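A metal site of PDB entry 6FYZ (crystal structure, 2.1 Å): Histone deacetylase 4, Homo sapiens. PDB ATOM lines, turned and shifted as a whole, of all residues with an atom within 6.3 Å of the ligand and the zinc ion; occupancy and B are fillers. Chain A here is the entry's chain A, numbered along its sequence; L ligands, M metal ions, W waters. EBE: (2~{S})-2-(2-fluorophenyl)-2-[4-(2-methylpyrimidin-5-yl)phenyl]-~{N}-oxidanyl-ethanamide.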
ATOM      1  N   PRO A  32      20.044 -20.686 -23.735  1.00  0.00           N
ATOM      2  CA  PRO A  32      21.167 -21.630 -23.550  1.00  0.00           C
ATOM      3  C   PRO A  32      21.639 -22.407 -24.800  1.00  0.00           C
ATOM      4  O   PRO A  32      22.756 -22.931 -24.796  1.00  0.00           O
ATOM      5  CB  PRO A  32      20.648 -22.588 -22.466  1.00  0.00           C
ATOM      6  CG  PRO A  32      19.166 -22.467 -22.509  1.00  0.00           C
ATOM      7  CD  PRO A  32      18.862 -21.067 -22.944  1.00  0.00           C
ATOM      8  N   GLU A  33      20.815 -22.462 -25.843  1.00  0.00           N
ATOM      9  CA  GLU A  33      21.253 -23.012 -27.124  1.00  0.00           C
ATOM     10  C   GLU A  33      21.808 -21.872 -27.985  1.00  0.00           C
ATOM     11  O   GLU A  33      21.120 -21.337 -28.845  1.00  0.00           O
ATOM     12  CB  GLU A  33      20.105 -23.768 -27.819  1.00  0.00           C
ATOM     13  CG  GLU A  33      20.572 -24.820 -28.827  1.00  0.00           C
ATOM     14  CD  GLU A  33      21.359 -24.238 -29.992  1.00  0.00           C
ATOM     15  OE1 GLU A  33      20.701 -23.830 -30.992  1.00  0.00           O
ATOM     16  OE2 GLU A  33      22.609 -24.181 -29.902  1.00  0.00           O
ATOM     17  N   HIS A  34      23.087 -21.532 -27.768  1.00  0.00           N
ATOM     18  CA  HIS A  34      23.726 -20.355 -28.372  1.00  0.00           C
ATOM     19  C   HIS A  34      24.967 -20.670 -29.227  1.00  0.00           C
ATOM     20  O   HIS A  34      25.584 -21.738 -29.081  1.00  0.00           O
ATOM     21  CB  HIS A  34      24.091 -19.325 -27.283  1.00  0.00           C
ATOM     22  CG  HIS A  34      25.104 -19.810 -26.303  1.00  0.00           C
ATOM     23  ND1 HIS A  34      26.449 -19.541 -26.427  1.00  0.00           N
ATOM     24  CD2 HIS A  34      24.975 -20.573 -25.188  1.00  0.00           C
ATOM     25  CE1 HIS A  34      27.108 -20.122 -25.435  1.00  0.00           C
ATOM     26  NE2 HIS A  34      26.230 -20.748 -24.675  1.00  0.00           N
ATOM     27  N   ARG A  37      28.437 -22.418 -28.369  1.00  0.00           N
ATOM     28  CA  ARG A  37      28.568 -23.870 -28.211  1.00  0.00           C
ATOM     29  C   ARG A  37      29.441 -24.479 -29.313  1.00  0.00           C
ATOM     30  O   ARG A  37      30.397 -25.186 -29.007  1.00  0.00           O
ATOM     31  CB  ARG A  37      27.186 -24.539 -28.197  1.00  0.00           C
ATOM     32  CG  ARG A  37      26.297 -24.152 -27.026  1.00  0.00           C
ATOM     33  CD  ARG A  37      24.897 -24.718 -27.171  1.00  0.00           C
ATOM     34  NE  ARG A  37      24.949 -26.179 -27.167  1.00  0.00           N
ATOM     35  CZ  ARG A  37      24.573 -26.988 -28.150  1.00  0.00           C
ATOM     36  NH1 ARG A  37      24.714 -28.307 -27.984  1.00  0.00           N
ATOM     37  NH2 ARG A  37      24.039 -26.533 -29.285  1.00  0.00           N
ATOM     38  N   PRO A 156      20.280 -28.126 -32.583  1.00  0.00           N
ATOM     39  CA  PRO A 156      20.136 -29.575 -32.432  1.00  0.00           C
ATOM     40  C   PRO A 156      18.859 -30.097 -33.109  1.00  0.00           C
ATOM     41  O   PRO A 156      18.000 -29.306 -33.520  1.00  0.00           O
ATOM     42  CB  PRO A 156      20.056 -29.748 -30.922  1.00  0.00           C
ATOM     43  CG  PRO A 156      19.430 -28.485 -30.458  1.00  0.00           C
ATOM     44  CD  PRO A 156      19.978 -27.421 -31.331  1.00  0.00           C
ATOM     45  N   HIS A 158      17.166 -33.674 -32.297  1.00  0.00           N
ATOM     46  CA  HIS A 158      16.508 -34.910 -31.868  1.00  0.00           C
ATOM     47  C   HIS A 158      15.104 -34.764 -31.251  1.00  0.00           C
ATOM     48  O   HIS A 158      14.355 -35.738 -31.221  1.00  0.00           O
ATOM     49  CB  HIS A 158      17.464 -35.780 -31.036  1.00  0.00           C
ATOM     50  CG  HIS A 158      17.704 -35.331 -29.625  1.00  0.00           C
ATOM     51  ND1 HIS A 158      18.008 -36.206 -28.618  1.00  0.00           N
ATOM     52  CD2 HIS A 158      17.693 -34.085 -29.062  1.00  0.00           C
ATOM     53  CE1 HIS A 158      18.174 -35.542 -27.493  1.00  0.00           C
ATOM     54  NE2 HIS A 158      17.989 -34.251 -27.733  1.00  0.00           N
ATOM     55  N   HIS A 159      14.729 -33.552 -30.796  1.00  0.00           N
ATOM     56  CA  HIS A 159      13.361 -33.307 -30.335  1.00  0.00           C
ATOM     57  C   HIS A 159      12.361 -32.906 -31.434  1.00  0.00           C
ATOM     58  O   HIS A 159      11.153 -32.869 -31.169  1.00  0.00           O
ATOM     59  CB  HIS A 159      13.330 -32.232 -29.249  1.00  0.00           C
ATOM     60  CG  HIS A 159      14.093 -32.591 -28.009  1.00  0.00           C
ATOM     61  ND1 HIS A 159      13.853 -33.743 -27.298  1.00  0.00           N
ATOM     62  CD2 HIS A 159      15.066 -31.930 -27.353  1.00  0.00           C
ATOM     63  CE1 HIS A 159      14.663 -33.782 -26.252  1.00  0.00           C
ATOM     64  NE2 HIS A 159      15.416 -32.689 -26.268  1.00  0.00           N
ATOM     65  N   MET A 166      10.506 -28.544 -31.052  1.00  0.00           N
ATOM     66  CA  MET A 166      10.575 -28.390 -29.582  1.00  0.00           C
ATOM     67  C   MET A 166      11.986 -28.585 -29.075  1.00  0.00           C
ATOM     68  O   MET A 166      12.858 -29.041 -29.808  1.00  0.00           O
ATOM     69  CB  MET A 166       9.609 -29.338 -28.839  1.00  0.00           C
ATOM     70  CG  MET A 166       9.664 -30.789 -29.271  1.00  0.00           C
ATOM     71  SD  MET A 166       8.927 -31.907 -28.040  1.00  0.00           S
ATOM     72  CE  MET A 166      10.183 -31.924 -26.770  1.00  0.00           C
ATOM     73  N   GLY A 167      12.202 -28.175 -27.833  1.00  0.00           N
ATOM     74  CA  GLY A 167      13.502 -28.326 -27.185  1.00  0.00           C
ATOM     75  C   GLY A 167      14.654 -27.719 -27.964  1.00  0.00           C
ATOM     76  O   GLY A 167      15.728 -28.303 -28.042  1.00  0.00           O
ATOM     77  N   PHE A 168      14.408 -26.537 -28.532  1.00  0.00           N
ATOM     78  CA  PHE A 168      15.397 -25.818 -29.372  1.00  0.00           C
ATOM     79  C   PHE A 168      15.775 -26.534 -30.684  1.00  0.00           C
ATOM     80  O   PHE A 168      16.793 -26.199 -31.280  1.00  0.00           O
ATOM     81  CB  PHE A 168      16.661 -25.453 -28.575  1.00  0.00           C
ATOM     82  CG  PHE A 168      16.382 -24.881 -27.204  1.00  0.00           C
ATOM     83  CD1 PHE A 168      15.417 -23.883 -27.018  1.00  0.00           C
ATOM     84  CD2 PHE A 168      17.125 -25.310 -26.100  1.00  0.00           C
ATOM     85  CE1 PHE A 168      15.179 -23.356 -25.752  1.00  0.00           C
ATOM     86  CE2 PHE A 168      16.893 -24.770 -24.830  1.00  0.00           C
ATOM     87  CZ  PHE A 168      15.916 -23.794 -24.661  1.00  0.00           C
ATOM     88  N   CYS A 169      14.946 -27.485 -31.133  1.00  0.00           N
ATOM     89  CA  CYS A 169      15.151 -28.225 -32.381  1.00  0.00           C
ATOM     90  C   CYS A 169      14.039 -27.893 -33.371  1.00  0.00           C
ATOM     91  O   CYS A 169      12.881 -27.709 -32.977  1.00  0.00           O
ATOM     92  CB  CYS A 169      15.162 -29.746 -32.126  1.00  0.00           C
ATOM     93  SG  CYS A 169      16.233 -30.327 -30.794  1.00  0.00           S
ATOM     94  N   ASP A 196      22.635 -38.183 -25.713  1.00  0.00           N
ATOM     95  CA  ASP A 196      22.147 -36.970 -25.088  1.00  0.00           C
ATOM     96  C   ASP A 196      21.339 -37.412 -23.862  1.00  0.00           C
ATOM     97  O   ASP A 196      20.670 -38.454 -23.878  1.00  0.00           O
ATOM     98  CB  ASP A 196      21.286 -36.188 -26.075  1.00  0.00           C
ATOM     99  CG  ASP A 196      20.928 -34.820 -25.573  1.00  0.00           C
ATOM    100  OD1 ASP A 196      20.079 -34.731 -24.664  1.00  0.00           O
ATOM    101  OD2 ASP A 196      21.486 -33.821 -26.109  1.00  0.00           O
ATOM    102  N   VAL A 197      21.413 -36.639 -22.774  1.00  0.00           N
ATOM    103  CA  VAL A 197      20.761 -37.024 -21.510  1.00  0.00           C
ATOM    104  C   VAL A 197      19.225 -36.930 -21.565  1.00  0.00           C
ATOM    105  O   VAL A 197      18.546 -37.501 -20.702  1.00  0.00           O
ATOM    106  CB  VAL A 197      21.335 -36.212 -20.315  1.00  0.00           C
ATOM    107  CG1 VAL A 197      20.709 -34.828 -20.223  1.00  0.00           C
ATOM    108  CG2 VAL A 197      21.165 -36.973 -19.014  1.00  0.00           C
ATOM    109  N   HIS A 198      18.697 -36.224 -22.563  1.00  0.00           N
ATOM    110  CA  HIS A 198      17.245 -36.171 -22.801  1.00  0.00           C
ATOM    111  C   HIS A 198      16.823 -37.137 -23.916  1.00  0.00           C
ATOM    112  O   HIS A 198      17.601 -37.403 -24.830  1.00  0.00           O
ATOM    113  CB  HIS A 198      16.803 -34.744 -23.154  1.00  0.00           C
ATOM    114  CG  HIS A 198      17.316 -33.713 -22.201  1.00  0.00           C
ATOM    115  ND1 HIS A 198      18.439 -32.974 -22.452  1.00  0.00           N
ATOM    116  CD2 HIS A 198      16.850 -33.306 -20.996  1.00  0.00           C
ATOM    117  CE1 HIS A 198      18.670 -32.159 -21.436  1.00  0.00           C
ATOM    118  NE2 HIS A 198      17.702 -32.325 -20.547  1.00  0.00           N
ATOM    119  N   HIS A 199      15.602 -37.647 -23.834  1.00  0.00           N
ATOM    120  CA  HIS A 199      15.062 -38.564 -24.839  1.00  0.00           C
ATOM    121  C   HIS A 199      14.847 -37.841 -26.177  1.00  0.00           C
ATOM    122  O   HIS A 199      14.241 -36.771 -26.196  1.00  0.00           O
ATOM    123  CB  HIS A 199      13.720 -39.124 -24.362  1.00  0.00           C
ATOM    124  CG  HIS A 199      13.083 -40.105 -25.298  1.00  0.00           C
ATOM    125  ND1 HIS A 199      11.800 -39.959 -25.780  1.00  0.00           N
ATOM    126  CD2 HIS A 199      13.550 -41.261 -25.835  1.00  0.00           C
ATOM    127  CE1 HIS A 199      11.502 -40.980 -26.569  1.00  0.00           C
ATOM    128  NE2 HIS A 199      12.552 -41.776 -26.617  1.00  0.00           N
ATOM    129  N   PHE A 227      12.585 -34.054 -18.546  1.00  0.00           N
ATOM    130  CA  PHE A 227      12.345 -33.470 -19.852  1.00  0.00           C
ATOM    131  C   PHE A 227      12.847 -34.416 -20.963  1.00  0.00           C
ATOM    132  O   PHE A 227      13.989 -34.852 -20.889  1.00  0.00           O
ATOM    133  CB  PHE A 227      13.045 -32.114 -19.982  1.00  0.00           C
ATOM    134  CG  PHE A 227      12.845 -31.474 -21.322  1.00  0.00           C
ATOM    135  CD1 PHE A 227      11.731 -30.698 -21.566  1.00  0.00           C
ATOM    136  CD2 PHE A 227      13.755 -31.696 -22.350  1.00  0.00           C
ATOM    137  CE1 PHE A 227      11.528 -30.127 -22.812  1.00  0.00           C
ATOM    138  CE2 PHE A 227      13.561 -31.125 -23.584  1.00  0.00           C
ATOM    139  CZ  PHE A 227      12.446 -30.349 -23.828  1.00  0.00           C
ATOM    140  N   GLY A 288      24.666 -35.623 -27.792  1.00  0.00           N
ATOM    141  CA  GLY A 288      24.578 -34.551 -26.805  1.00  0.00           C
ATOM    142  C   GLY A 288      25.571 -34.810 -25.677  1.00  0.00           C
ATOM    143  O   GLY A 288      25.807 -35.951 -25.316  1.00  0.00           O
ATOM    144  N   ASP A 290      25.307 -33.323 -22.523  1.00  0.00           N
ATOM    145  CA  ASP A 290      24.675 -32.754 -21.323  1.00  0.00           C
ATOM    146  C   ASP A 290      24.543 -33.741 -20.148  1.00  0.00           C
ATOM    147  O   ASP A 290      24.119 -33.339 -19.067  1.00  0.00           O
ATOM    148  CB  ASP A 290      23.334 -32.055 -21.657  1.00  0.00           C
ATOM    149  CG  ASP A 290      22.431 -32.873 -22.573  1.00  0.00           C
ATOM    150  OD1 ASP A 290      22.690 -34.071 -22.782  1.00  0.00           O
ATOM    151  OD2 ASP A 290      21.442 -32.300 -23.077  1.00  0.00           O
ATOM    152  N   PRO A 298      17.242 -28.661 -15.087  1.00  0.00           N
ATOM    153  CA  PRO A 298      16.861 -29.791 -15.945  1.00  0.00           C
ATOM    154  C   PRO A 298      17.648 -29.945 -17.263  1.00  0.00           C
ATOM    155  O   PRO A 298      17.191 -30.677 -18.156  1.00  0.00           O
ATOM    156  CB  PRO A 298      15.397 -29.464 -16.239  1.00  0.00           C
ATOM    157  CG  PRO A 298      15.387 -27.980 -16.358  1.00  0.00           C
ATOM    158  CD  PRO A 298      16.478 -27.457 -15.443  1.00  0.00           C
ATOM    159  N   LEU A 299      18.785 -29.276 -17.398  1.00  0.00           N
ATOM    160  CA  LEU A 299      19.671 -29.461 -18.552  1.00  0.00           C
ATOM    161  C   LEU A 299      20.478 -30.749 -18.437  1.00  0.00           C
ATOM    162  O   LEU A 299      20.985 -31.253 -19.438  1.00  0.00           O
ATOM    163  CB  LEU A 299      20.622 -28.281 -18.717  1.00  0.00           C
ATOM    164  CG  LEU A 299      19.988 -26.909 -18.953  1.00  0.00           C
ATOM    165  CD1 LEU A 299      21.036 -25.817 -18.823  1.00  0.00           C
ATOM    166  CD2 LEU A 299      19.295 -26.858 -20.300  1.00  0.00           C
ATOM    167  N   GLU A 329      24.167 -32.758 -30.348  1.00  0.00           N
ATOM    168  CA  GLU A 329      22.794 -32.473 -30.002  1.00  0.00           C
ATOM    169  C   GLU A 329      22.855 -31.445 -28.861  1.00  0.00           C
ATOM    170  O   GLU A 329      23.225 -30.290 -29.125  1.00  0.00           O
ATOM    171  CB  GLU A 329      22.025 -33.748 -29.654  1.00  0.00           C
ATOM    172  CG  GLU A 329      21.871 -34.736 -30.821  1.00  0.00           C
ATOM    173  CD  GLU A 329      20.803 -34.357 -31.846  1.00  0.00           C
ATOM    174  OE1 GLU A 329      20.166 -33.289 -31.733  1.00  0.00           O
ATOM    175  OE2 GLU A 329      20.606 -35.146 -32.791  1.00  0.00           O
ATOM    176  N   GLY A 330      22.528 -31.838 -27.630  1.00  0.00           N
ATOM    177  CA  GLY A 330      22.586 -30.948 -26.468  1.00  0.00           C
ATOM    178  C   GLY A 330      23.968 -30.830 -25.860  1.00  0.00           C
ATOM    179  O   GLY A 330      24.979 -31.216 -26.469  1.00  0.00           O
ATOM    180  N   GLY A 331      24.019 -30.283 -24.652  1.00  0.00           N
ATOM    181  CA  GLY A 331      25.293 -29.937 -24.016  1.00  0.00           C
ATOM    182  C   GLY A 331      25.465 -28.442 -24.099  1.00  0.00           C
ATOM    183  O   GLY A 331      25.474 -27.852 -25.179  1.00  0.00           O
ATOM    184  N   HIS A 332      25.643 -27.843 -22.920  1.00  0.00           N
ATOM    185  CA  HIS A 332      25.527 -26.404 -22.683  1.00  0.00           C
ATOM    186  C   HIS A 332      26.834 -25.818 -22.121  1.00  0.00           C
ATOM    187  O   HIS A 332      27.360 -24.822 -22.650  1.00  0.00           O
ATOM    188  CB  HIS A 332      24.365 -26.190 -21.717  1.00  0.00           C
ATOM    189  CG  HIS A 332      24.290 -24.817 -21.142  1.00  0.00           C
ATOM    190  ND1 HIS A 332      23.772 -23.752 -21.836  1.00  0.00           N
ATOM    191  CD2 HIS A 332      24.661 -24.343 -19.934  1.00  0.00           C
ATOM    192  CE1 HIS A 332      23.845 -22.669 -21.085  1.00  0.00           C
ATOM    193  NE2 HIS A 332      24.369 -23.003 -19.926  1.00  0.00           N
HETATM  194  C4  EBE L   1      15.928 -28.175 -24.472  1.00  0.00           C
HETATM  195  C5  EBE L   1      14.962 -27.915 -23.500  1.00  0.00           C
HETATM  196  C6  EBE L   1      15.135 -28.302 -22.161  1.00  0.00           C
HETATM  197  C7  EBE L   1      14.085 -28.018 -21.103  1.00  0.00           C
HETATM  198  C8  EBE L   1      12.984 -27.178 -21.359  1.00  0.00           C
HETATM  199  C3  EBE L   1      17.099 -28.833 -24.148  1.00  0.00           C
HETATM  200  C2  EBE L   1      17.295 -29.217 -22.827  1.00  0.00           C
HETATM  201  C10 EBE L   1      12.169 -27.476 -19.173  1.00  0.00           C
HETATM  202  C1  EBE L   1      16.332 -28.969 -21.848  1.00  0.00           C
HETATM  203  C19 EBE L   1      19.493 -27.189 -24.174  1.00  0.00           C
HETATM  204  C12 EBE L   1      14.155 -28.561 -19.806  1.00  0.00           C
HETATM  205  C13 EBE L   1      18.119 -29.081 -25.217  1.00  0.00           C
HETATM  206  C14 EBE L   1      19.267 -28.122 -25.193  1.00  0.00           C
HETATM  207  C18 EBE L   1      20.591 -26.340 -24.217  1.00  0.00           C
HETATM  208  N9  EBE L   1      12.060 -26.943 -20.402  1.00  0.00           N
HETATM  209  C20 EBE L   1      18.649 -30.499 -25.107  1.00  0.00           C
HETATM  210  C24 EBE L   1      11.123 -27.198 -18.127  1.00  0.00           C
HETATM  211  O21 EBE L   1      19.714 -30.731 -24.550  1.00  0.00           O
HETATM  212  N22 EBE L   1      17.927 -31.471 -25.659  1.00  0.00           N
HETATM  213  O23 EBE L   1      18.360 -32.792 -25.589  1.00  0.00           O
HETATM  214  C17 EBE L   1      21.476 -26.396 -25.281  1.00  0.00           C
HETATM  215  C16 EBE L   1      21.269 -27.326 -26.288  1.00  0.00           C
HETATM  216  C15 EBE L   1      20.172 -28.172 -26.254  1.00  0.00           C
HETATM  217  F25 EBE L   1      20.015 -29.063 -27.257  1.00  0.00           F
HETATM  218  N11 EBE L   1      13.214 -28.287 -18.891  1.00  0.00           N
HETATM  219 ZN    ZN M   1      19.754 -32.875 -24.058  1.00  0.00          ZN
HETATM  220  O   HOH W   1      21.798 -29.324 -23.089  1.00  0.00           O
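NE2 of His 158 lies within hydrogen-bond range of N22 of the ligand. A nitrogen (N22) of the ligand is in hydrogen-bond range of a ring nitrogen (NE2) of His 159 (2.9 Å).
O of Pro 298 sits at hydrogen-bond distance from NE2 of His 198 (2.9 Å). A ring nitrogen (NE2) of His 158 lies within hydrogen-bond range of a ring nitrogen (NE2) of His 159 (3.3 Å). The backbone NH (N) of His 158 lies within hydrogen-bond range of the side-chain carboxylate (OE1) of Glu 329, 3.1 Å away. N of His 159 is in hydrogen-bond range of SG of Cys 169, 3.6 Å away. The guanidinium group of Arg 37 lies within hydrogen-bond range of the backbone carbonyl oxygen of Gly 330. OE2 of Glu 33 is in salt-bridge range of NH2 of Arg 37 (2.8 Å). NH1 of Arg 37 is in hydrogen-bond range of O of Glu 329, 2.7 Å away. The backbone carbonyl oxygen (O) of Gly 331 lies within hydrogen-bond range of the guanidinium group (NE) of Arg 37.
Residues that only touch the ligand: Gly 330, Pro 156, Pro 298, Phe 227, Phe 168, Gly 167, Glu 33, Pro 32, Arg 37, Leu 299 and Glu 329. Hydrophobic or aromatic side chains within 4 Å of the ligand: Pro 156, His 158, His 159, Phe 168, His 198, Phe 227, Pro 298 and Leu 299. 16 residues have an atom within 4 Å of the ligand: Pro 32, Glu 33, Arg 37, Pro 156, His 158, His 159, Gly 167, Phe 168, Asp 196, His 198, Phe 227, Asp 290, Pro 298, Leu 299, Glu 329 and Gly 330. The nearest printed residue that does not touch the ligand is Gly 331 (4.3 Å).
OD1 of Asp 196 is bound to the zinc ion, at 2.0 Å. OD2 of Asp 290 binds the zinc ion. The zinc ion is bound by O23 of the ligand, 2.1 Å away. A ring nitrogen (ND1) of His 198 is bound to the zinc ion (2.1 Å). The zinc ion is bound by an oxygen (O21) of the ligand, at 2.2 Å. Slightly farther from the zinc ion lies the side-chain carboxylate (OD2) of Asp 196 (2.8 Å).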
